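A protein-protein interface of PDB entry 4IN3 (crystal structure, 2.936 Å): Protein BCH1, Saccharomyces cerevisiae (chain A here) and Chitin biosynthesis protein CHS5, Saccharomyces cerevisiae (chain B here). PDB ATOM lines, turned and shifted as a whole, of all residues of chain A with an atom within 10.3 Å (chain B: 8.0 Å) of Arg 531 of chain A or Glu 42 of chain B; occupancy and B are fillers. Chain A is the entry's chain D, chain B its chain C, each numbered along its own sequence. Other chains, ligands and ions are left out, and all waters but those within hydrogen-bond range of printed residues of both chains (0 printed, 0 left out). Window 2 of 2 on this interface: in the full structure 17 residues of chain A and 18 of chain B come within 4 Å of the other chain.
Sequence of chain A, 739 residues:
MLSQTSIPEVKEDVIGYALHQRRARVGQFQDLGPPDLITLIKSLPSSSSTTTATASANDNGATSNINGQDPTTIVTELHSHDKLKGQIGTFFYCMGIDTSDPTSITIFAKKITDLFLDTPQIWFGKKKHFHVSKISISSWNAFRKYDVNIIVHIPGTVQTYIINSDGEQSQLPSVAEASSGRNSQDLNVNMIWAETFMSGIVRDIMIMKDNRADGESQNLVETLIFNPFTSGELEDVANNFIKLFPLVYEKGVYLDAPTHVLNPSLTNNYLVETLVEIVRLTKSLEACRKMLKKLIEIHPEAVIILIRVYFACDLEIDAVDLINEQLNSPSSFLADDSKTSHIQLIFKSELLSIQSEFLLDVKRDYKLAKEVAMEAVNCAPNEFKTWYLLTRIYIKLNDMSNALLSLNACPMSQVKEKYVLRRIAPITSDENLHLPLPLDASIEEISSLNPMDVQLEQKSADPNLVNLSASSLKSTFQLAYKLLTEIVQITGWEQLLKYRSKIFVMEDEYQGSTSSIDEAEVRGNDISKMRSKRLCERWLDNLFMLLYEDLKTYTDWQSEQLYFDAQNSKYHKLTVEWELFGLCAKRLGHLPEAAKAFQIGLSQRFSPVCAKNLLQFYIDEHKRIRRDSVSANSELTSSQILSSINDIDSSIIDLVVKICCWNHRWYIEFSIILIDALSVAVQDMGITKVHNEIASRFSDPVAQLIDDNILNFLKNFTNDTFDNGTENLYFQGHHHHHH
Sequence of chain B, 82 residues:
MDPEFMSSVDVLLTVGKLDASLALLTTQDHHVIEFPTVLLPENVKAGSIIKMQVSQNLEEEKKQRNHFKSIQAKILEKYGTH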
ATOM      1  N   LEU A 405      18.183   5.239 -19.230  1.00  0.00           N
ATOM      2  CA  LEU A 405      16.775   5.409 -19.559  1.00  0.00           C
ATOM      3  C   LEU A 405      16.625   6.170 -20.870  1.00  0.00           C
ATOM      4  O   LEU A 405      15.774   5.846 -21.697  1.00  0.00           O
ATOM      5  CB  LEU A 405      16.046   6.148 -18.436  1.00  0.00           C
ATOM      6  CG  LEU A 405      15.896   5.390 -17.115  1.00  0.00           C
ATOM      7  CD1 LEU A 405      14.919   6.104 -16.194  1.00  0.00           C
ATOM      8  CD2 LEU A 405      15.454   3.956 -17.366  1.00  0.00           C
ATOM      9  N   SER A 501      20.787  -3.410 -13.666  1.00  0.00           N
ATOM     10  CA  SER A 501      19.927  -4.384 -13.013  1.00  0.00           C
ATOM     11  C   SER A 501      18.812  -3.703 -12.222  1.00  0.00           C
ATOM     12  O   SER A 501      17.766  -4.303 -11.978  1.00  0.00           O
ATOM     13  CB  SER A 501      20.753  -5.297 -12.102  1.00  0.00           C
ATOM     14  OG  SER A 501      20.138  -6.563 -11.949  1.00  0.00           O
ATOM     15  N   LYS A 502      19.034  -2.447 -11.837  1.00  0.00           N
ATOM     16  CA  LYS A 502      18.062  -1.705 -11.027  1.00  0.00           C
ATOM     17  C   LYS A 502      16.944  -1.049 -11.838  1.00  0.00           C
ATOM     18  O   LYS A 502      15.950  -0.594 -11.274  1.00  0.00           O
ATOM     19  CB  LYS A 502      18.756  -0.636 -10.177  1.00  0.00           C
ATOM     20  CG  LYS A 502      19.595  -1.188  -9.040  1.00  0.00           C
ATOM     21  CD  LYS A 502      19.382  -0.377  -7.768  1.00  0.00           C
ATOM     22  CE  LYS A 502      20.684   0.206  -7.237  1.00  0.00           C
ATOM     23  NZ  LYS A 502      20.683   1.697  -7.286  1.00  0.00           N
ATOM     24  N   ILE A 503      17.104  -0.990 -13.155  1.00  0.00           N
ATOM     25  CA  ILE A 503      16.106  -0.345 -14.000  1.00  0.00           C
ATOM     26  C   ILE A 503      15.632  -1.240 -15.144  1.00  0.00           C
ATOM     27  O   ILE A 503      14.596  -0.969 -15.761  1.00  0.00           O
ATOM     28  CB  ILE A 503      16.629   0.977 -14.588  1.00  0.00           C
ATOM     29  CG1 ILE A 503      17.980   0.755 -15.268  1.00  0.00           C
ATOM     30  CG2 ILE A 503      16.736   2.045 -13.506  1.00  0.00           C
ATOM     31  CD1 ILE A 503      18.591   2.013 -15.838  1.00  0.00           C
ATOM     32  N   PHE A 504      16.385  -2.299 -15.429  1.00  0.00           N
ATOM     33  CA  PHE A 504      16.047  -3.175 -16.547  1.00  0.00           C
ATOM     34  C   PHE A 504      15.591  -4.566 -16.099  1.00  0.00           C
ATOM     35  O   PHE A 504      15.749  -4.937 -14.939  1.00  0.00           O
ATOM     36  CB  PHE A 504      17.186  -3.226 -17.572  1.00  0.00           C
ATOM     37  CG  PHE A 504      17.402  -1.920 -18.287  1.00  0.00           C
ATOM     38  CD1 PHE A 504      16.349  -1.031 -18.455  1.00  0.00           C
ATOM     39  CD2 PHE A 504      18.643  -1.578 -18.789  1.00  0.00           C
ATOM     40  CE1 PHE A 504      16.528   0.173 -19.110  1.00  0.00           C
ATOM     41  CE2 PHE A 504      18.830  -0.371 -19.449  1.00  0.00           C
ATOM     42  CZ  PHE A 504      17.772   0.504 -19.609  1.00  0.00           C
ATOM     43  N   VAL A 505      15.041  -5.332 -17.038  1.00  0.00           N
ATOM     44  CA  VAL A 505      14.243  -6.520 -16.722  1.00  0.00           C
ATOM     45  C   VAL A 505      15.039  -7.816 -16.510  1.00  0.00           C
ATOM     46  O   VAL A 505      14.444  -8.873 -16.286  1.00  0.00           O
ATOM     47  CB  VAL A 505      13.172  -6.780 -17.792  1.00  0.00           C
ATOM     48  CG1 VAL A 505      12.153  -5.637 -17.838  1.00  0.00           C
ATOM     49  CG2 VAL A 505      13.819  -6.987 -19.157  1.00  0.00           C
ATOM     50  N   MET A 506      16.361  -7.754 -16.599  1.00  0.00           N
ATOM     51  CA  MET A 506      17.212  -8.882 -16.206  1.00  0.00           C
ATOM     52  C   MET A 506      16.931 -10.218 -16.908  1.00  0.00           C
ATOM     53  O   MET A 506      16.830 -10.286 -18.133  1.00  0.00           O
ATOM     54  CB  MET A 506      17.155  -9.078 -14.688  1.00  0.00           C
ATOM     55  CG  MET A 506      15.756  -9.323 -14.146  1.00  0.00           C
ATOM     56  SD  MET A 506      15.052  -7.867 -13.350  1.00  0.00           S
ATOM     57  CE  MET A 506      16.378  -7.417 -12.234  1.00  0.00           C
ATOM     58  N   MET A 530      10.253  -5.733 -10.100  1.00  0.00           N
ATOM     59  CA  MET A 530       9.247  -6.403 -10.917  1.00  0.00           C
ATOM     60  C   MET A 530       8.480  -5.417 -11.801  1.00  0.00           C
ATOM     61  O   MET A 530       8.254  -5.674 -12.985  1.00  0.00           O
ATOM     62  CB  MET A 530       8.270  -7.182 -10.026  1.00  0.00           C
ATOM     63  CG  MET A 530       7.742  -6.373  -8.843  1.00  0.00           C
ATOM     64  SD  MET A 530       6.305  -7.107  -8.042  1.00  0.00           S
ATOM     65  CE  MET A 530       5.460  -5.626  -7.492  1.00  0.00           C
ATOM     66  N   ARG A 531       8.093  -4.283 -11.221  1.00  0.00           N
ATOM     67  CA  ARG A 531       7.233  -3.316 -11.898  1.00  0.00           C
ATOM     68  C   ARG A 531       7.996  -2.138 -12.501  1.00  0.00           C
ATOM     69  O   ARG A 531       8.033  -1.972 -13.722  1.00  0.00           O
ATOM     70  CB  ARG A 531       6.177  -2.788 -10.923  1.00  0.00           C
ATOM     71  CG  ARG A 531       4.981  -2.108 -11.578  1.00  0.00           C
ATOM     72  CD  ARG A 531       3.761  -3.011 -11.526  1.00  0.00           C
ATOM     73  NE  ARG A 531       2.562  -2.371 -12.060  1.00  0.00           N
ATOM     74  CZ  ARG A 531       1.478  -3.037 -12.448  1.00  0.00           C
ATOM     75  NH1 ARG A 531       1.454  -4.360 -12.371  1.00  0.00           N
ATOM     76  NH2 ARG A 531       0.426  -2.385 -12.922  1.00  0.00           N
ATOM     77  N   SER A 532       8.602  -1.328 -11.634  1.00  0.00           N
ATOM     78  CA  SER A 532       9.280  -0.097 -12.042  1.00  0.00           C
ATOM     79  C   SER A 532      10.427  -0.337 -13.025  1.00  0.00           C
ATOM     80  O   SER A 532      10.871   0.589 -13.713  1.00  0.00           O
ATOM     81  CB  SER A 532       9.784   0.676 -10.818  1.00  0.00           C
ATOM     82  OG  SER A 532      10.480   1.847 -11.216  1.00  0.00           O
ATOM     83  N   LYS A 533      10.908  -1.574 -13.084  1.00  0.00           N
ATOM     84  CA  LYS A 533      11.912  -1.932 -14.072  1.00  0.00           C
ATOM     85  C   LYS A 533      11.259  -1.969 -15.451  1.00  0.00           C
ATOM     86  O   LYS A 533      10.176  -2.534 -15.616  1.00  0.00           O
ATOM     87  CB  LYS A 533      12.533  -3.290 -13.743  1.00  0.00           C
ATOM     88  CG  LYS A 533      13.008  -3.437 -12.304  1.00  0.00           C
ATOM     89  CD  LYS A 533      14.332  -4.181 -12.249  1.00  0.00           C
ATOM     90  CE  LYS A 533      14.285  -5.372 -11.312  1.00  0.00           C
ATOM     91  NZ  LYS A 533      13.102  -6.232 -11.597  1.00  0.00           N
ATOM     92  N   ARG A 534      11.923  -1.386 -16.446  1.00  0.00           N
ATOM     93  CA  ARG A 534      11.378  -1.384 -17.798  1.00  0.00           C
ATOM     94  C   ARG A 534      12.218  -2.278 -18.711  1.00  0.00           C
ATOM     95  O   ARG A 534      13.214  -2.862 -18.279  1.00  0.00           O
ATOM     96  CB  ARG A 534      11.279   0.039 -18.353  1.00  0.00           C
ATOM     97  CG  ARG A 534      12.616   0.700 -18.646  1.00  0.00           C
ATOM     98  CD  ARG A 534      12.432   2.151 -19.053  1.00  0.00           C
ATOM     99  NE  ARG A 534      11.904   2.963 -17.961  1.00  0.00           N
ATOM    100  CZ  ARG A 534      11.641   4.263 -18.053  1.00  0.00           C
ATOM    101  NH1 ARG A 534      11.854   4.906 -19.194  1.00  0.00           N
ATOM    102  NH2 ARG A 534      11.163   4.918 -17.004  1.00  0.00           N
ATOM    103  N   LEU A 535      11.813  -2.388 -19.970  1.00  0.00           N
ATOM    104  CA  LEU A 535      12.433  -3.348 -20.872  1.00  0.00           C
ATOM    105  C   LEU A 535      13.650  -2.777 -21.585  1.00  0.00           C
ATOM    106  O   LEU A 535      13.589  -1.681 -22.140  1.00  0.00           O
ATOM    107  CB  LEU A 535      11.418  -3.817 -21.912  1.00  0.00           C
ATOM    108  CG  LEU A 535      11.953  -4.778 -22.972  1.00  0.00           C
ATOM    109  CD1 LEU A 535      12.422  -6.074 -22.324  1.00  0.00           C
ATOM    110  CD2 LEU A 535      10.928  -5.051 -24.066  1.00  0.00           C
ATOM    111  N   LEU B  18      -0.437  -8.569 -21.480  1.00  0.00           N
ATOM    112  CA  LEU B  18       0.231  -7.748 -20.476  1.00  0.00           C
ATOM    113  C   LEU B  18       1.617  -8.280 -20.099  1.00  0.00           C
ATOM    114  O   LEU B  18       1.742  -9.416 -19.638  1.00  0.00           O
ATOM    115  CB  LEU B  18      -0.669  -7.653 -19.238  1.00  0.00           C
ATOM    116  CG  LEU B  18      -0.360  -6.686 -18.093  1.00  0.00           C
ATOM    117  CD1 LEU B  18       0.426  -7.360 -16.979  1.00  0.00           C
ATOM    118  CD2 LEU B  18       0.364  -5.450 -18.593  1.00  0.00           C
ATOM    119  N   ASP B  19       2.653  -7.461 -20.291  1.00  0.00           N
ATOM    120  CA  ASP B  19       3.998  -7.822 -19.840  1.00  0.00           C
ATOM    121  C   ASP B  19       4.630  -6.736 -18.956  1.00  0.00           C
ATOM    122  O   ASP B  19       4.059  -5.665 -18.780  1.00  0.00           O
ATOM    123  CB  ASP B  19       4.902  -8.196 -21.031  1.00  0.00           C
ATOM    124  CG  ASP B  19       5.260  -7.007 -21.910  1.00  0.00           C
ATOM    125  OD1 ASP B  19       6.251  -6.314 -21.599  1.00  0.00           O
ATOM    126  OD2 ASP B  19       4.565  -6.782 -22.923  1.00  0.00           O
ATOM    127  N   ALA B  20       5.827  -7.005 -18.439  1.00  0.00           N
ATOM    128  CA  ALA B  20       6.484  -6.118 -17.472  1.00  0.00           C
ATOM    129  C   ALA B  20       6.844  -4.740 -18.029  1.00  0.00           C
ATOM    130  O   ALA B  20       7.218  -3.835 -17.278  1.00  0.00           O
ATOM    131  CB  ALA B  20       7.731  -6.792 -16.893  1.00  0.00           C
ATOM    132  N   SER B  21       6.745  -4.573 -19.339  1.00  0.00           N
ATOM    133  CA  SER B  21       6.883  -3.249 -19.914  1.00  0.00           C
ATOM    134  C   SER B  21       5.516  -2.720 -20.336  1.00  0.00           C
ATOM    135  O   SER B  21       5.044  -1.696 -19.842  1.00  0.00           O
ATOM    136  CB  SER B  21       7.834  -3.292 -21.111  1.00  0.00           C
ATOM    137  OG  SER B  21       7.959  -2.013 -21.715  1.00  0.00           O
ATOM    138  N   ALA B  23       1.314  -2.839 -21.614  1.00  0.00           N
ATOM    139  CA  ALA B  23      -0.061  -3.287 -21.573  1.00  0.00           C
ATOM    140  C   ALA B  23      -0.725  -2.856 -22.873  1.00  0.00           C
ATOM    141  O   ALA B  23      -0.340  -1.858 -23.484  1.00  0.00           O
ATOM    142  CB  ALA B  23      -0.779  -2.671 -20.395  1.00  0.00           C
ATOM    143  N   PRO B  36       2.499   1.747 -20.896  1.00  0.00           N
ATOM    144  CA  PRO B  36       3.491   1.111 -20.018  1.00  0.00           C
ATOM    145  C   PRO B  36       2.804   0.580 -18.759  1.00  0.00           C
ATOM    146  O   PRO B  36       1.852   1.196 -18.275  1.00  0.00           O
ATOM    147  CB  PRO B  36       4.443   2.259 -19.671  1.00  0.00           C
ATOM    148  CG  PRO B  36       3.595   3.481 -19.763  1.00  0.00           C
ATOM    149  CD  PRO B  36       2.574   3.218 -20.847  1.00  0.00           C
ATOM    150  N   THR B  37       3.273  -0.550 -18.240  1.00  0.00           N
ATOM    151  CA  THR B  37       2.619  -1.193 -17.104  1.00  0.00           C
ATOM    152  C   THR B  37       2.845  -0.425 -15.802  1.00  0.00           C
ATOM    153  O   THR B  37       2.024  -0.492 -14.887  1.00  0.00           O
ATOM    154  CB  THR B  37       3.087  -2.655 -16.924  1.00  0.00           C
ATOM    155  OG1 THR B  37       3.203  -3.289 -18.206  1.00  0.00           O
ATOM    156  CG2 THR B  37       2.103  -3.429 -16.057  1.00  0.00           C
ATOM    157  N   VAL B  38       3.951   0.310 -15.727  1.00  0.00           N
ATOM    158  CA  VAL B  38       4.312   1.008 -14.497  1.00  0.00           C
ATOM    159  C   VAL B  38       3.403   2.210 -14.219  1.00  0.00           C
ATOM    160  O   VAL B  38       3.368   2.723 -13.098  1.00  0.00           O
ATOM    161  CB  VAL B  38       5.800   1.437 -14.499  1.00  0.00           C
ATOM    162  CG1 VAL B  38       6.006   2.682 -15.339  1.00  0.00           C
ATOM    163  CG2 VAL B  38       6.298   1.641 -13.079  1.00  0.00           C
ATOM    164  N   LEU B  39       2.664   2.652 -15.235  1.00  0.00           N
ATOM    165  CA  LEU B  39       1.675   3.714 -15.048  1.00  0.00           C
ATOM    166  C   LEU B  39       0.314   3.115 -14.691  1.00  0.00           C
ATOM    167  O   LEU B  39      -0.695   3.819 -14.650  1.00  0.00           O
ATOM    168  CB  LEU B  39       1.561   4.602 -16.293  1.00  0.00           C
ATOM    169  CG  LEU B  39       2.483   5.824 -16.376  1.00  0.00           C
ATOM    170  CD1 LEU B  39       3.936   5.414 -16.541  1.00  0.00           C
ATOM    171  CD2 LEU B  39       2.052   6.739 -17.514  1.00  0.00           C
ATOM    172  N   LEU B  40       0.303   1.811 -14.431  1.00  0.00           N
ATOM    173  CA  LEU B  40      -0.906   1.101 -14.042  1.00  0.00           C
ATOM    174  C   LEU B  40      -0.755   0.586 -12.614  1.00  0.00           C
ATOM    175  O   LEU B  40       0.357   0.286 -12.179  1.00  0.00           O
ATOM    176  CB  LEU B  40      -1.160  -0.068 -14.995  1.00  0.00           C
ATOM    177  CG  LEU B  40      -1.336   0.307 -16.468  1.00  0.00           C
ATOM    178  CD1 LEU B  40      -1.544  -0.940 -17.317  1.00  0.00           C
ATOM    179  CD2 LEU B  40      -2.502   1.270 -16.626  1.00  0.00           C
ATOM    180  N   PRO B  41      -1.876   0.495 -11.875  1.00  0.00           N
ATOM    181  CA  PRO B  41      -1.888  -0.034 -10.503  1.00  0.00           C
ATOM    182  C   PRO B  41      -1.275  -1.440 -10.395  1.00  0.00           C
ATOM    183  O   PRO B  41      -1.322  -2.216 -11.353  1.00  0.00           O
ATOM    184  CB  PRO B  41      -3.383  -0.060 -10.153  1.00  0.00           C
ATOM    185  CG  PRO B  41      -3.971   1.034 -10.982  1.00  0.00           C
ATOM    186  CD  PRO B  41      -3.189   1.035 -12.269  1.00  0.00           C
ATOM    187  N   GLU B  42      -0.725  -1.752  -9.223  1.00  0.00           N
ATOM    188  CA  GLU B  42       0.063  -2.967  -8.984  1.00  0.00           C
ATOM    189  C   GLU B  42      -0.629  -4.334  -9.140  1.00  0.00           C
ATOM    190  O   GLU B  42       0.013  -5.303  -9.541  1.00  0.00           O
ATOM    191  CB  GLU B  42       0.691  -2.878  -7.593  1.00  0.00           C
ATOM    192  CG  GLU B  42      -0.214  -2.158  -6.608  1.00  0.00           C
ATOM    193  CD  GLU B  42       0.071  -2.504  -5.165  1.00  0.00           C
ATOM    194  OE1 GLU B  42       1.244  -2.760  -4.818  1.00  0.00           O
ATOM    195  OE2 GLU B  42      -0.890  -2.518  -4.371  1.00  0.00           O
ATOM    196  N   ASN B  43      -1.920  -4.389  -8.833  1.00  0.00           N
ATOM    197  CA  ASN B  43      -2.701  -5.605  -9.023  1.00  0.00           C
ATOM    198  C   ASN B  43      -3.557  -5.493 -10.278  1.00  0.00           C
ATOM    199  O   ASN B  43      -4.774  -5.670 -10.230  1.00  0.00           O
ATOM    200  CB  ASN B  43      -3.583  -5.873  -7.803  1.00  0.00           C
ATOM    201  CG  ASN B  43      -2.778  -6.078  -6.535  1.00  0.00           C
ATOM    202  OD1 ASN B  43      -1.553  -6.181  -6.573  1.00  0.00           O
ATOM    203  ND2 ASN B  43      -3.467  -6.139  -5.401  1.00  0.00           N
ATOM    204  N   VAL B  44      -2.911  -5.189 -11.398  1.00  0.00           N
ATOM    205  CA  VAL B  44      -3.614  -4.943 -12.652  1.00  0.00           C
ATOM    206  C   VAL B  44      -3.968  -6.219 -13.410  1.00  0.00           C
ATOM    207  O   VAL B  44      -5.007  -6.284 -14.068  1.00  0.00           O
ATOM    208  CB  VAL B  44      -2.800  -4.021 -13.580  1.00  0.00           C
ATOM    209  CG1 VAL B  44      -1.488  -4.684 -13.968  1.00  0.00           C
ATOM    210  CG2 VAL B  44      -3.610  -3.666 -14.816  1.00  0.00           C
ATOM    211  N   LYS B  45      -3.107  -7.235 -13.324  1.00  0.00           N
ATOM    212  CA  LYS B  45      -3.323  -8.509 -14.048  1.00  0.00           C
ATOM    213  C   LYS B  45      -3.625  -8.354 -15.554  1.00  0.00           C
ATOM    214  O   LYS B  45      -3.009  -7.548 -16.253  1.00  0.00           O
ATOM    215  CB  LYS B  45      -4.463  -9.298 -13.379  1.00  0.00           C
ATOM    216  CG  LYS B  45      -4.192 -10.792 -13.199  1.00  0.00           C
ATOM    217  CD  LYS B  45      -5.477 -11.550 -12.886  1.00  0.00           C
ATOM    218  CE  LYS B  45      -6.247 -10.925 -11.726  1.00  0.00           C
ATOM    219  NZ  LYS B  45      -7.555 -11.604 -11.474  1.00  0.00           N
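The guanidinium group (NH2) of Arg 531 of chain A lies within hydrogen-bond range of the backbone carbonyl oxygen (O) of Thr 37 of chain B.
The backbone carbonyl oxygen of Pro 41 of chain B sits close to the guanidinium group of Arg 531 of chain A, at 2.4 Å.
O of Glu 42 of chain B is in hydrogen-bond range of NH1 of Arg 531 of chain A, 3.3 Å away.
NH2 of Arg 531 of chain A sits at hydrogen-bond distance from O of Leu 40 of chain B, at 2.8 Å.
The side-chain hydroxyl (OG1) of Thr 37 of chain B is in hydrogen-bond range of the backbone carbonyl oxygen (O) of Asp 19 of chain B (2.6 Å).
N of Ser 21 of chain B sits at hydrogen-bond distance from OD1 of Asp 19 of chain B (2.9 Å).
SD of Met 506 of chain A sits at hydrogen-bond distance from NZ of Lys 533 of chain A (3.1 Å).
The backbone carbonyl oxygen (O) of Ser 21 of chain B lies within hydrogen-bond range of the backbone NH (N) of Thr 37 of chain B, 2.6 Å away.
Among the printed residues, pairs that only touch across the chains: Arg 531 of chain A with Val 44 of chain B (3.2 Å), Ser 532 of chain A with Val 38 of chain B (3.6 Å), Lys 533 of chain A with Ala 20 of chain B (3.6 Å) and Leu 535 of chain A with Ser 21 of chain B (3.7 Å).
Ile 503 of chain A touches none of the printed residues of chain B.
Of chain B, only Thr 37, Leu 40, Pro 41, Glu 42 and Val 44 come within 4 Å of Arg 531 of chain A.
Of the printed residues of chain B, Lys 533 of chain A touches Ala 20 (3.6 Å).
Arg 534 of chain A touches none of the printed residues of chain B.
Printed residues of chain B within 4 Å of Leu 535 of chain A: Ser 21 (3.7 Å).
Printed residues of chain A within 4 Å of Ala 20 of chain B: Lys 533.
Leu 40 of chain B touches one residue of chain A.
Of chain A, only Arg 531 comes within 4 Å of Glu 42 of chain B.
No residue of chain A comes within 4 Å of Asn 43 of chain B.
The nearest residue of chain B that does not touch Arg 531 of chain A is Val 38 of chain B (4.1 Å).
The nearest printed residue of chain A that does not touch Val 44 of chain B is Met 530 of chain A (9.2 Å).
Of the 13 printed residues of chain A, 4 touch a printed residue of chain B.
Hydrophobic or aromatic side chains of chain A that line the printed part of chain B: Leu 535.
Of the 15 printed residues of chain B, 8 touch a printed residue of chain A.
Hydrophobic or aromatic side chains of chain B within 4 Å of the printed part of chain A: Val 38, Leu 40 and Val 44.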
